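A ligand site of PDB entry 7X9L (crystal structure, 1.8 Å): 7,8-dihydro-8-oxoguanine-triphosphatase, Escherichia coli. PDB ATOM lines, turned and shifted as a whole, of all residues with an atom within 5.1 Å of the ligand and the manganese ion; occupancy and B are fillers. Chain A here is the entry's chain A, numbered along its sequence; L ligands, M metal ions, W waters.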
ATOM      1  N   ILE A   6     -10.906 -13.674  11.302  1.00  0.00           N
ATOM      2  CA  ILE A   6     -11.800 -12.519  11.388  1.00  0.00           C
ATOM      3  C   ILE A   6     -12.831 -12.617  10.266  1.00  0.00           C
ATOM      4  O   ILE A   6     -12.466 -12.865   9.113  1.00  0.00           O
ATOM      5  CB  ILE A   6     -11.026 -11.190  11.283  1.00  0.00           C
ATOM      6  CG1 ILE A   6      -9.924 -11.083  12.349  1.00  0.00           C
ATOM      7  CG2 ILE A   6     -11.982 -10.002  11.339  1.00  0.00           C
ATOM      8  CD1 ILE A   6     -10.434 -11.188  13.786  1.00  0.00           C
ATOM      9  N   VAL A   8     -15.798 -10.457   8.237  1.00  0.00           N
ATOM     10  CA  VAL A   8     -16.317  -9.106   8.021  1.00  0.00           C
ATOM     11  C   VAL A   8     -17.338  -9.141   6.887  1.00  0.00           C
ATOM     12  O   VAL A   8     -17.327 -10.018   6.018  1.00  0.00           O
ATOM     13  CB  VAL A   8     -15.188  -8.081   7.726  1.00  0.00           C
ATOM     14  CG1 VAL A   8     -14.043  -8.249   8.697  1.00  0.00           C
ATOM     15  CG2 VAL A   8     -14.693  -8.208   6.299  1.00  0.00           C
ATOM     16  N   ARG A  23     -12.948   2.618  13.034  1.00  0.00           N
ATOM     17  CA  ARG A  23     -12.439   1.959  14.220  1.00  0.00           C
ATOM     18  C   ARG A  23     -12.001   2.953  15.288  1.00  0.00           C
ATOM     19  O   ARG A  23     -11.579   4.065  14.980  1.00  0.00           O
ATOM     20  CB  ARG A  23     -11.270   1.039  13.845  1.00  0.00           C
ATOM     21  CG  ARG A  23     -11.688  -0.098  12.936  1.00  0.00           C
ATOM     22  CD  ARG A  23     -10.533  -0.999  12.546  1.00  0.00           C
ATOM     23  NE  ARG A  23      -9.901  -1.649  13.690  1.00  0.00           N
ATOM     24  CZ  ARG A  23     -10.368  -2.735  14.298  1.00  0.00           C
ATOM     25  NH1 ARG A  23     -11.508  -3.303  13.889  1.00  0.00           N
ATOM     26  NH2 ARG A  23      -9.708  -3.241  15.330  1.00  0.00           N
ATOM     27  N   HIS A  28      -6.653  -1.834  17.697  1.00  0.00           N
ATOM     28  CA  HIS A  28      -5.744  -2.192  16.632  1.00  0.00           C
ATOM     29  C   HIS A  28      -6.271  -1.589  15.336  1.00  0.00           C
ATOM     30  O   HIS A  28      -7.482  -1.511  15.134  1.00  0.00           O
ATOM     31  CB  HIS A  28      -5.627  -3.716  16.526  1.00  0.00           C
ATOM     32  CG  HIS A  28      -4.651  -4.169  15.478  1.00  0.00           C
ATOM     33  ND1 HIS A  28      -5.053  -4.795  14.321  1.00  0.00           N
ATOM     34  CD2 HIS A  28      -3.310  -4.036  15.407  1.00  0.00           C
ATOM     35  CE1 HIS A  28      -3.988  -5.049  13.575  1.00  0.00           C
ATOM     36  NE2 HIS A  28      -2.912  -4.597  14.214  1.00  0.00           N
ATOM     37  N   MET A  29      -5.361  -1.123  14.479  1.00  0.00           N
ATOM     38  CA  MET A  29      -5.751  -0.393  13.266  1.00  0.00           C
ATOM     39  C   MET A  29      -6.646   0.802  13.628  1.00  0.00           C
ATOM     40  O   MET A  29      -7.723   1.006  13.067  1.00  0.00           O
ATOM     41  CB  MET A  29      -6.428  -1.319  12.259  1.00  0.00           C
ATOM     42  CG  MET A  29      -5.456  -2.235  11.539  1.00  0.00           C
ATOM     43  SD  MET A  29      -4.284  -1.285  10.531  1.00  0.00           S
ATOM     44  CE  MET A  29      -2.786  -1.412  11.500  1.00  0.00           C
ATOM     45  N   GLU A  34     -13.453   0.563   8.005  1.00  0.00           N
ATOM     46  CA  GLU A  34     -13.492  -0.887   8.079  1.00  0.00           C
ATOM     47  C   GLU A  34     -14.824  -1.416   7.578  1.00  0.00           C
ATOM     48  O   GLU A  34     -15.839  -0.705   7.589  1.00  0.00           O
ATOM     49  CB  GLU A  34     -13.269  -1.379   9.524  1.00  0.00           C
ATOM     50  CG  GLU A  34     -14.320  -0.826  10.504  1.00  0.00           C
ATOM     51  CD  GLU A  34     -14.415  -1.599  11.817  1.00  0.00           C
ATOM     52  OE1 GLU A  34     -13.599  -2.515  12.059  1.00  0.00           O
ATOM     53  OE2 GLU A  34     -15.320  -1.258  12.617  1.00  0.00           O
ATOM     54  N   PHE A  35     -14.815  -2.659   7.124  1.00  0.00           N
ATOM     55  CA  PHE A  35     -16.065  -3.425   7.032  1.00  0.00           C
ATOM     56  C   PHE A  35     -16.415  -3.960   8.416  1.00  0.00           C
ATOM     57  O   PHE A  35     -15.551  -4.509   9.104  1.00  0.00           O
ATOM     58  CB  PHE A  35     -15.894  -4.587   6.050  1.00  0.00           C
ATOM     59  CG  PHE A  35     -15.370  -4.180   4.710  1.00  0.00           C
ATOM     60  CD1 PHE A  35     -16.088  -3.308   3.907  1.00  0.00           C
ATOM     61  CD2 PHE A  35     -14.155  -4.674   4.256  1.00  0.00           C
ATOM     62  CE1 PHE A  35     -15.601  -2.933   2.653  1.00  0.00           C
ATOM     63  CE2 PHE A  35     -13.664  -4.322   3.011  1.00  0.00           C
ATOM     64  CZ  PHE A  35     -14.370  -3.432   2.204  1.00  0.00           C
ATOM     65  N   PRO A  36     -17.662  -3.828   8.873  1.00  0.00           N
ATOM     66  CA  PRO A  36     -18.007  -4.362  10.202  1.00  0.00           C
ATOM     67  C   PRO A  36     -17.674  -5.843  10.287  1.00  0.00           C
ATOM     68  O   PRO A  36     -17.848  -6.587   9.315  1.00  0.00           O
ATOM     69  CB  PRO A  36     -19.512  -4.110  10.315  1.00  0.00           C
ATOM     70  CG  PRO A  36     -19.748  -2.913   9.388  1.00  0.00           C
ATOM     71  CD  PRO A  36     -18.813  -3.175   8.231  1.00  0.00           C
ATOM     72  N   GLY A  37     -17.177  -6.278  11.439  1.00  0.00           N
ATOM     73  CA  GLY A  37     -16.819  -7.676  11.624  1.00  0.00           C
ATOM     74  C   GLY A  37     -16.027  -7.883  12.893  1.00  0.00           C
ATOM     75  O   GLY A  37     -15.877  -6.965  13.708  1.00  0.00           O
ATOM     76  N   GLY A  38     -15.535  -9.102  13.057  1.00  0.00           N
ATOM     77  CA  GLY A  38     -14.769  -9.442  14.247  1.00  0.00           C
ATOM     78  C   GLY A  38     -14.400 -10.903  14.258  1.00  0.00           C
ATOM     79  O   GLY A  38     -14.548 -11.620  13.267  1.00  0.00           O
ATOM     80  N   LYS A  39     -13.929 -11.343  15.429  1.00  0.00           N
ATOM     81  CA  LYS A  39     -13.276 -12.643  15.527  1.00  0.00           C
ATOM     82  C   LYS A  39     -14.277 -13.787  15.448  1.00  0.00           C
ATOM     83  O   LYS A  39     -15.343 -13.745  16.063  1.00  0.00           O
ATOM     84  CB  LYS A  39     -12.494 -12.739  16.833  1.00  0.00           C
ATOM     85  CG  LYS A  39     -11.809 -14.086  17.024  1.00  0.00           C
ATOM     86  CD  LYS A  39     -11.373 -14.267  18.467  1.00  0.00           C
ATOM     87  CE  LYS A  39     -10.936 -15.707  18.719  1.00  0.00           C
ATOM     88  NZ  LYS A  39     -10.600 -15.945  20.163  1.00  0.00           N
ATOM     89  N   GLU A  53     -21.561 -11.029  14.037  1.00  0.00           N
ATOM     90  CA  GLU A  53     -20.831  -9.767  14.125  1.00  0.00           C
ATOM     91  C   GLU A  53     -21.634  -8.608  13.558  1.00  0.00           C
ATOM     92  O   GLU A  53     -21.604  -7.496  14.101  1.00  0.00           O
ATOM     93  CB  GLU A  53     -19.489  -9.898  13.415  1.00  0.00           C
ATOM     94  CG  GLU A  53     -18.473 -10.776  14.149  1.00  0.00           C
ATOM     95  CD  GLU A  53     -17.901 -10.095  15.376  1.00  0.00           C
ATOM     96  OE1 GLU A  53     -18.064  -8.852  15.502  1.00  0.00           O
ATOM     97  OE2 GLU A  53     -17.270 -10.779  16.213  1.00  0.00           O
ATOM     98  N   GLU A  57     -22.690  -5.384  15.637  1.00  0.00           N
ATOM     99  CA  GLU A  57     -22.026  -4.118  15.346  1.00  0.00           C
ATOM    100  C   GLU A  57     -22.957  -3.112  14.681  1.00  0.00           C
ATOM    101  O   GLU A  57     -22.869  -1.916  14.964  1.00  0.00           O
ATOM    102  CB  GLU A  57     -20.790  -4.348  14.480  1.00  0.00           C
ATOM    103  CG  GLU A  57     -19.671  -5.058  15.225  1.00  0.00           C
ATOM    104  CD  GLU A  57     -18.304  -4.702  14.729  1.00  0.00           C
ATOM    105  OE1 GLU A  57     -18.171  -4.179  13.598  1.00  0.00           O
ATOM    106  OE2 GLU A  57     -17.343  -4.949  15.475  1.00  0.00           O
ATOM    107  N   PHE A  75       0.429  -8.447  10.282  1.00  0.00           N
ATOM    108  CA  PHE A  75       0.652  -7.146  10.891  1.00  0.00           C
ATOM    109  C   PHE A  75       1.925  -7.188  11.738  1.00  0.00           C
ATOM    110  O   PHE A  75       2.484  -8.258  11.988  1.00  0.00           O
ATOM    111  CB  PHE A  75      -0.558  -6.768  11.752  1.00  0.00           C
ATOM    112  CG  PHE A  75      -1.780  -6.402  10.971  1.00  0.00           C
ATOM    113  CD1 PHE A  75      -1.906  -5.141  10.409  1.00  0.00           C
ATOM    114  CD2 PHE A  75      -2.834  -7.303  10.831  1.00  0.00           C
ATOM    115  CE1 PHE A  75      -3.044  -4.782   9.693  1.00  0.00           C
ATOM    116  CE2 PHE A  75      -3.974  -6.956  10.126  1.00  0.00           C
ATOM    117  CZ  PHE A  75      -4.086  -5.687   9.550  1.00  0.00           C
ATOM    118  N   ARG A  78       0.683  -9.299  14.917  1.00  0.00           N
ATOM    119  CA  ARG A  78      -0.322 -10.341  14.884  1.00  0.00           C
ATOM    120  C   ARG A  78      -0.531 -10.793  13.445  1.00  0.00           C
ATOM    121  O   ARG A  78      -0.294 -10.033  12.507  1.00  0.00           O
ATOM    122  CB  ARG A  78      -1.646  -9.872  15.502  1.00  0.00           C
ATOM    123  CG  ARG A  78      -2.331  -8.763  14.713  1.00  0.00           C
ATOM    124  CD  ARG A  78      -3.378  -8.109  15.579  1.00  0.00           C
ATOM    125  NE  ARG A  78      -2.738  -7.267  16.586  1.00  0.00           N
ATOM    126  CZ  ARG A  78      -3.340  -6.792  17.666  1.00  0.00           C
ATOM    127  NH1 ARG A  78      -4.615  -7.090  17.890  1.00  0.00           N
ATOM    128  NH2 ARG A  78      -2.687  -6.028  18.519  1.00  0.00           N
ATOM    129  N   ILE A  80      -3.496 -12.345  10.938  1.00  0.00           N
ATOM    130  CA  ILE A  80      -4.938 -12.563  10.851  1.00  0.00           C
ATOM    131  C   ILE A  80      -5.295 -13.154   9.490  1.00  0.00           C
ATOM    132  O   ILE A  80      -4.667 -12.880   8.471  1.00  0.00           O
ATOM    133  CB  ILE A  80      -5.761 -11.282  11.106  1.00  0.00           C
ATOM    134  CG1 ILE A  80      -5.667 -10.333   9.924  1.00  0.00           C
ATOM    135  CG2 ILE A  80      -5.356 -10.614  12.410  1.00  0.00           C
ATOM    136  CD1 ILE A  80      -6.640  -9.200  10.057  1.00  0.00           C
ATOM    137  N   LEU A  82      -8.596 -13.060   7.156  1.00  0.00           N
ATOM    138  CA  LEU A  82      -9.803 -12.273   6.991  1.00  0.00           C
ATOM    139  C   LEU A  82     -10.733 -12.951   6.002  1.00  0.00           C
ATOM    140  O   LEU A  82     -10.321 -13.308   4.893  1.00  0.00           O
ATOM    141  CB  LEU A  82      -9.479 -10.861   6.502  1.00  0.00           C
ATOM    142  CG  LEU A  82      -9.039  -9.853   7.559  1.00  0.00           C
ATOM    143  CD1 LEU A  82      -8.112  -8.828   6.932  1.00  0.00           C
ATOM    144  CD2 LEU A  82     -10.251  -9.153   8.175  1.00  0.00           C
ATOM    145  N   PHE A  84     -13.895 -12.085   3.892  1.00  0.00           N
ATOM    146  CA  PHE A  84     -14.683 -10.946   3.413  1.00  0.00           C
ATOM    147  C   PHE A  84     -15.948 -11.494   2.762  1.00  0.00           C
ATOM    148  O   PHE A  84     -15.871 -12.077   1.667  1.00  0.00           O
ATOM    149  CB  PHE A  84     -13.899 -10.101   2.418  1.00  0.00           C
ATOM    150  CG  PHE A  84     -12.682  -9.425   2.983  1.00  0.00           C
ATOM    151  CD1 PHE A  84     -12.752  -8.109   3.439  1.00  0.00           C
ATOM    152  CD2 PHE A  84     -11.450 -10.076   3.016  1.00  0.00           C
ATOM    153  CE1 PHE A  84     -11.628  -7.454   3.939  1.00  0.00           C
ATOM    154  CE2 PHE A  84     -10.317  -9.438   3.514  1.00  0.00           C
ATOM    155  CZ  PHE A  84     -10.417  -8.127   3.979  1.00  0.00           C
ATOM    156  N   PRO A 116      -7.392  -0.694   6.739  1.00  0.00           N
ATOM    157  CA  PRO A 116      -6.188  -1.453   7.053  1.00  0.00           C
ATOM    158  C   PRO A 116      -5.555  -1.979   5.771  1.00  0.00           C
ATOM    159  O   PRO A 116      -6.260  -2.239   4.779  1.00  0.00           O
ATOM    160  CB  PRO A 116      -6.701  -2.598   7.929  1.00  0.00           C
ATOM    161  CG  PRO A 116      -7.920  -2.028   8.566  1.00  0.00           C
ATOM    162  CD  PRO A 116      -8.564  -1.253   7.439  1.00  0.00           C
ATOM    163  N   ALA A 118      -4.464  -4.763   4.937  1.00  0.00           N
ATOM    164  CA  ALA A 118      -4.949  -6.079   4.542  1.00  0.00           C
ATOM    165  C   ALA A 118      -6.096  -5.973   3.539  1.00  0.00           C
ATOM    166  O   ALA A 118      -6.305  -6.899   2.744  1.00  0.00           O
ATOM    167  CB  ALA A 118      -5.414  -6.851   5.769  1.00  0.00           C
ATOM    168  N   ASN A 119      -6.865  -4.871   3.561  1.00  0.00           N
ATOM    169  CA  ASN A 119      -8.020  -4.704   2.699  1.00  0.00           C
ATOM    170  C   ASN A 119      -7.680  -4.267   1.274  1.00  0.00           C
ATOM    171  O   ASN A 119      -8.598  -4.198   0.445  1.00  0.00           O
ATOM    172  CB  ASN A 119      -8.984  -3.661   3.291  1.00  0.00           C
ATOM    173  CG  ASN A 119      -9.632  -4.138   4.576  1.00  0.00           C
ATOM    174  OD1 ASN A 119      -9.049  -4.927   5.312  1.00  0.00           O
ATOM    175  ND2 ASN A 119     -10.837  -3.641   4.848  1.00  0.00           N
HETATM  176  O1  LIG L   1     -11.105  -5.352  16.376  1.00  0.00           O
HETATM  177  P1  LIG L   1     -11.932  -6.507  15.879  1.00  0.00           P
HETATM  178  O2  LIG L   1     -12.528  -7.386  16.927  1.00  0.00           O
HETATM  179  O3  LIG L   1     -12.954  -6.043  14.821  1.00  0.00           O
HETATM  180  O4  LIG L   1     -10.862  -7.449  15.126  1.00  0.00           O
HETATM  181  C1  LIG L   1     -10.657  -7.279  13.720  1.00  0.00           C
HETATM  182  C2  LIG L   1      -9.178  -7.428  13.333  1.00  0.00           C
HETATM  183  O5  LIG L   1      -9.091  -7.556  11.917  1.00  0.00           O
HETATM  184  C3  LIG L   1      -8.354  -6.203  13.684  1.00  0.00           C
HETATM  185  O6  LIG L   1      -6.999  -6.603  13.882  1.00  0.00           O
HETATM  186  C4  LIG L   1      -8.389  -5.376  12.416  1.00  0.00           C
HETATM  187  C5  LIG L   1      -8.417  -6.446  11.335  1.00  0.00           C
HETATM  188  N1  LIG L   1      -9.148  -5.946  10.147  1.00  0.00           N
HETATM  189  C6  LIG L   1      -8.654  -5.688   8.940  1.00  0.00           C
HETATM  190  N2  LIG L   1      -9.536  -5.242   8.035  1.00  0.00           N
HETATM  191  C7  LIG L   1     -10.713  -5.232   8.728  1.00  0.00           C
HETATM  192  C8  LIG L   1     -12.022  -4.896   8.387  1.00  0.00           C
HETATM  193  O7  LIG L   1     -12.330  -4.472   7.223  1.00  0.00           O
HETATM  194  N3  LIG L   1     -12.990  -5.015   9.335  1.00  0.00           N
HETATM  195  C9  LIG L   1     -12.706  -5.440  10.570  1.00  0.00           C
HETATM  196  N4  LIG L   1     -13.692  -5.562  11.492  1.00  0.00           N
HETATM  197  N5  LIG L   1     -11.460  -5.776  10.932  1.00  0.00           N
HETATM  198  C10 LIG L   1     -10.450  -5.690  10.023  1.00  0.00           C
HETATM  199  O8  LIG L   1      -7.406  -5.824   8.695  1.00  0.00           O
HETATM  200 MN    MN M   1     -15.137  -5.466  15.108  1.00  0.00          MN
HETATM  201  O   HOH W   1     -12.292  -3.383  17.520  1.00  0.00           O
HETATM  202  O   HOH W   2      -8.611  -6.080  17.670  1.00  0.00           O
HETATM  203  O   HOH W   3      -6.811  -7.860  16.439  1.00  0.00           O
HETATM  204  O   HOH W   4     -14.904  -3.574  16.372  1.00  0.00           O
HETATM  205  O   HOH W   5     -12.114  -6.816  19.545  1.00  0.00           O
HETATM  206  O   HOH W   6     -15.438  -3.991  13.523  1.00  0.00           O
HETATM  207  O   HOH W   7     -15.061  -6.693  16.902  1.00  0.00           O
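Water W7 binds the manganese ion (2.2 Å).
O of Gly 37 binds the manganese ion, 2.2 Å away.
The manganese ion is bound by water W6 (2.2 Å).
The manganese ion is bound by O3 of the ligand (2.3 Å).
Water W4 is bound to the manganese ion (2.3 Å).
OE2 of Glu 57 binds the manganese ion, 2.3 Å away.
The manganese ion has six donor atoms within binding distance.
Residues that only touch the ligand: Pro 116 (3.4 Å), Phe 75 (3.4 Å), Val 8 (3.5 Å), Ile 80 (3.5 Å), Leu 82 (3.6 Å), Ile 6 (3.6 Å), Ala 118 (3.7 Å) and Gly 38 (3.9 Å).
14 residues have an atom within 4 Å of the ligand: Ile 6, Val 8, Arg 23, His 28, Glu 34, Phe 35, Gly 37, Gly 38, Phe 75, Ile 80, Leu 82, Pro 116, Ala 118 and Asn 119.
The nearest printed residue that does not touch the ligand is Pro 36 (4.2 Å).
The guanidinium group (NE) of Arg 23 sits at hydrogen-bond distance from the backbone carbonyl oxygen (O) of His 28, at 2.8 Å.
NH1 of Arg 23 is in salt-bridge range of OE1 of Glu 34 (2.9 Å).
NE of Arg 23 sits at hydrogen-bond distance from O of Met 29.
Within 4 Å of the manganese ion: Gly 37 and Glu 57.
Water W6 lies within hydrogen-bond range of OE1 of Glu 57 (2.7 Å), OE1 of Glu 34 (2.8 Å) and N4 of the ligand (3.1 Å).
Water W1 lies within hydrogen-bond range of O1 of the ligand (2.6 Å) and NH2 of Arg 23 (3.4 Å).
Water W3 bridges the guanidinium group (NH1) of Arg 78 (2.7 Å) and an oxygen (O6) of the ligand (2.9 Å).
N of Phe 35 lies within hydrogen-bond range of O7 of the ligand (3.1 Å).
O of Phe 35 sits at hydrogen-bond distance from N3 of the ligand (2.6 Å).
A ring nitrogen (ND1) of His 28 is in hydrogen-bond range of an oxygen (O6) of the ligand, at 2.7 Å.
NH2 of Arg 23 lies within salt-bridge range of O1 of the ligand, 2.7 Å away.
A nitrogen (N2) of the ligand lies within hydrogen-bond range of the side-chain amide oxygen (OD1) of Asn 119, at 2.8 Å.
OE1 of Glu 34 lies within hydrogen-bond range of N4 of the ligand (3.1 Å).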
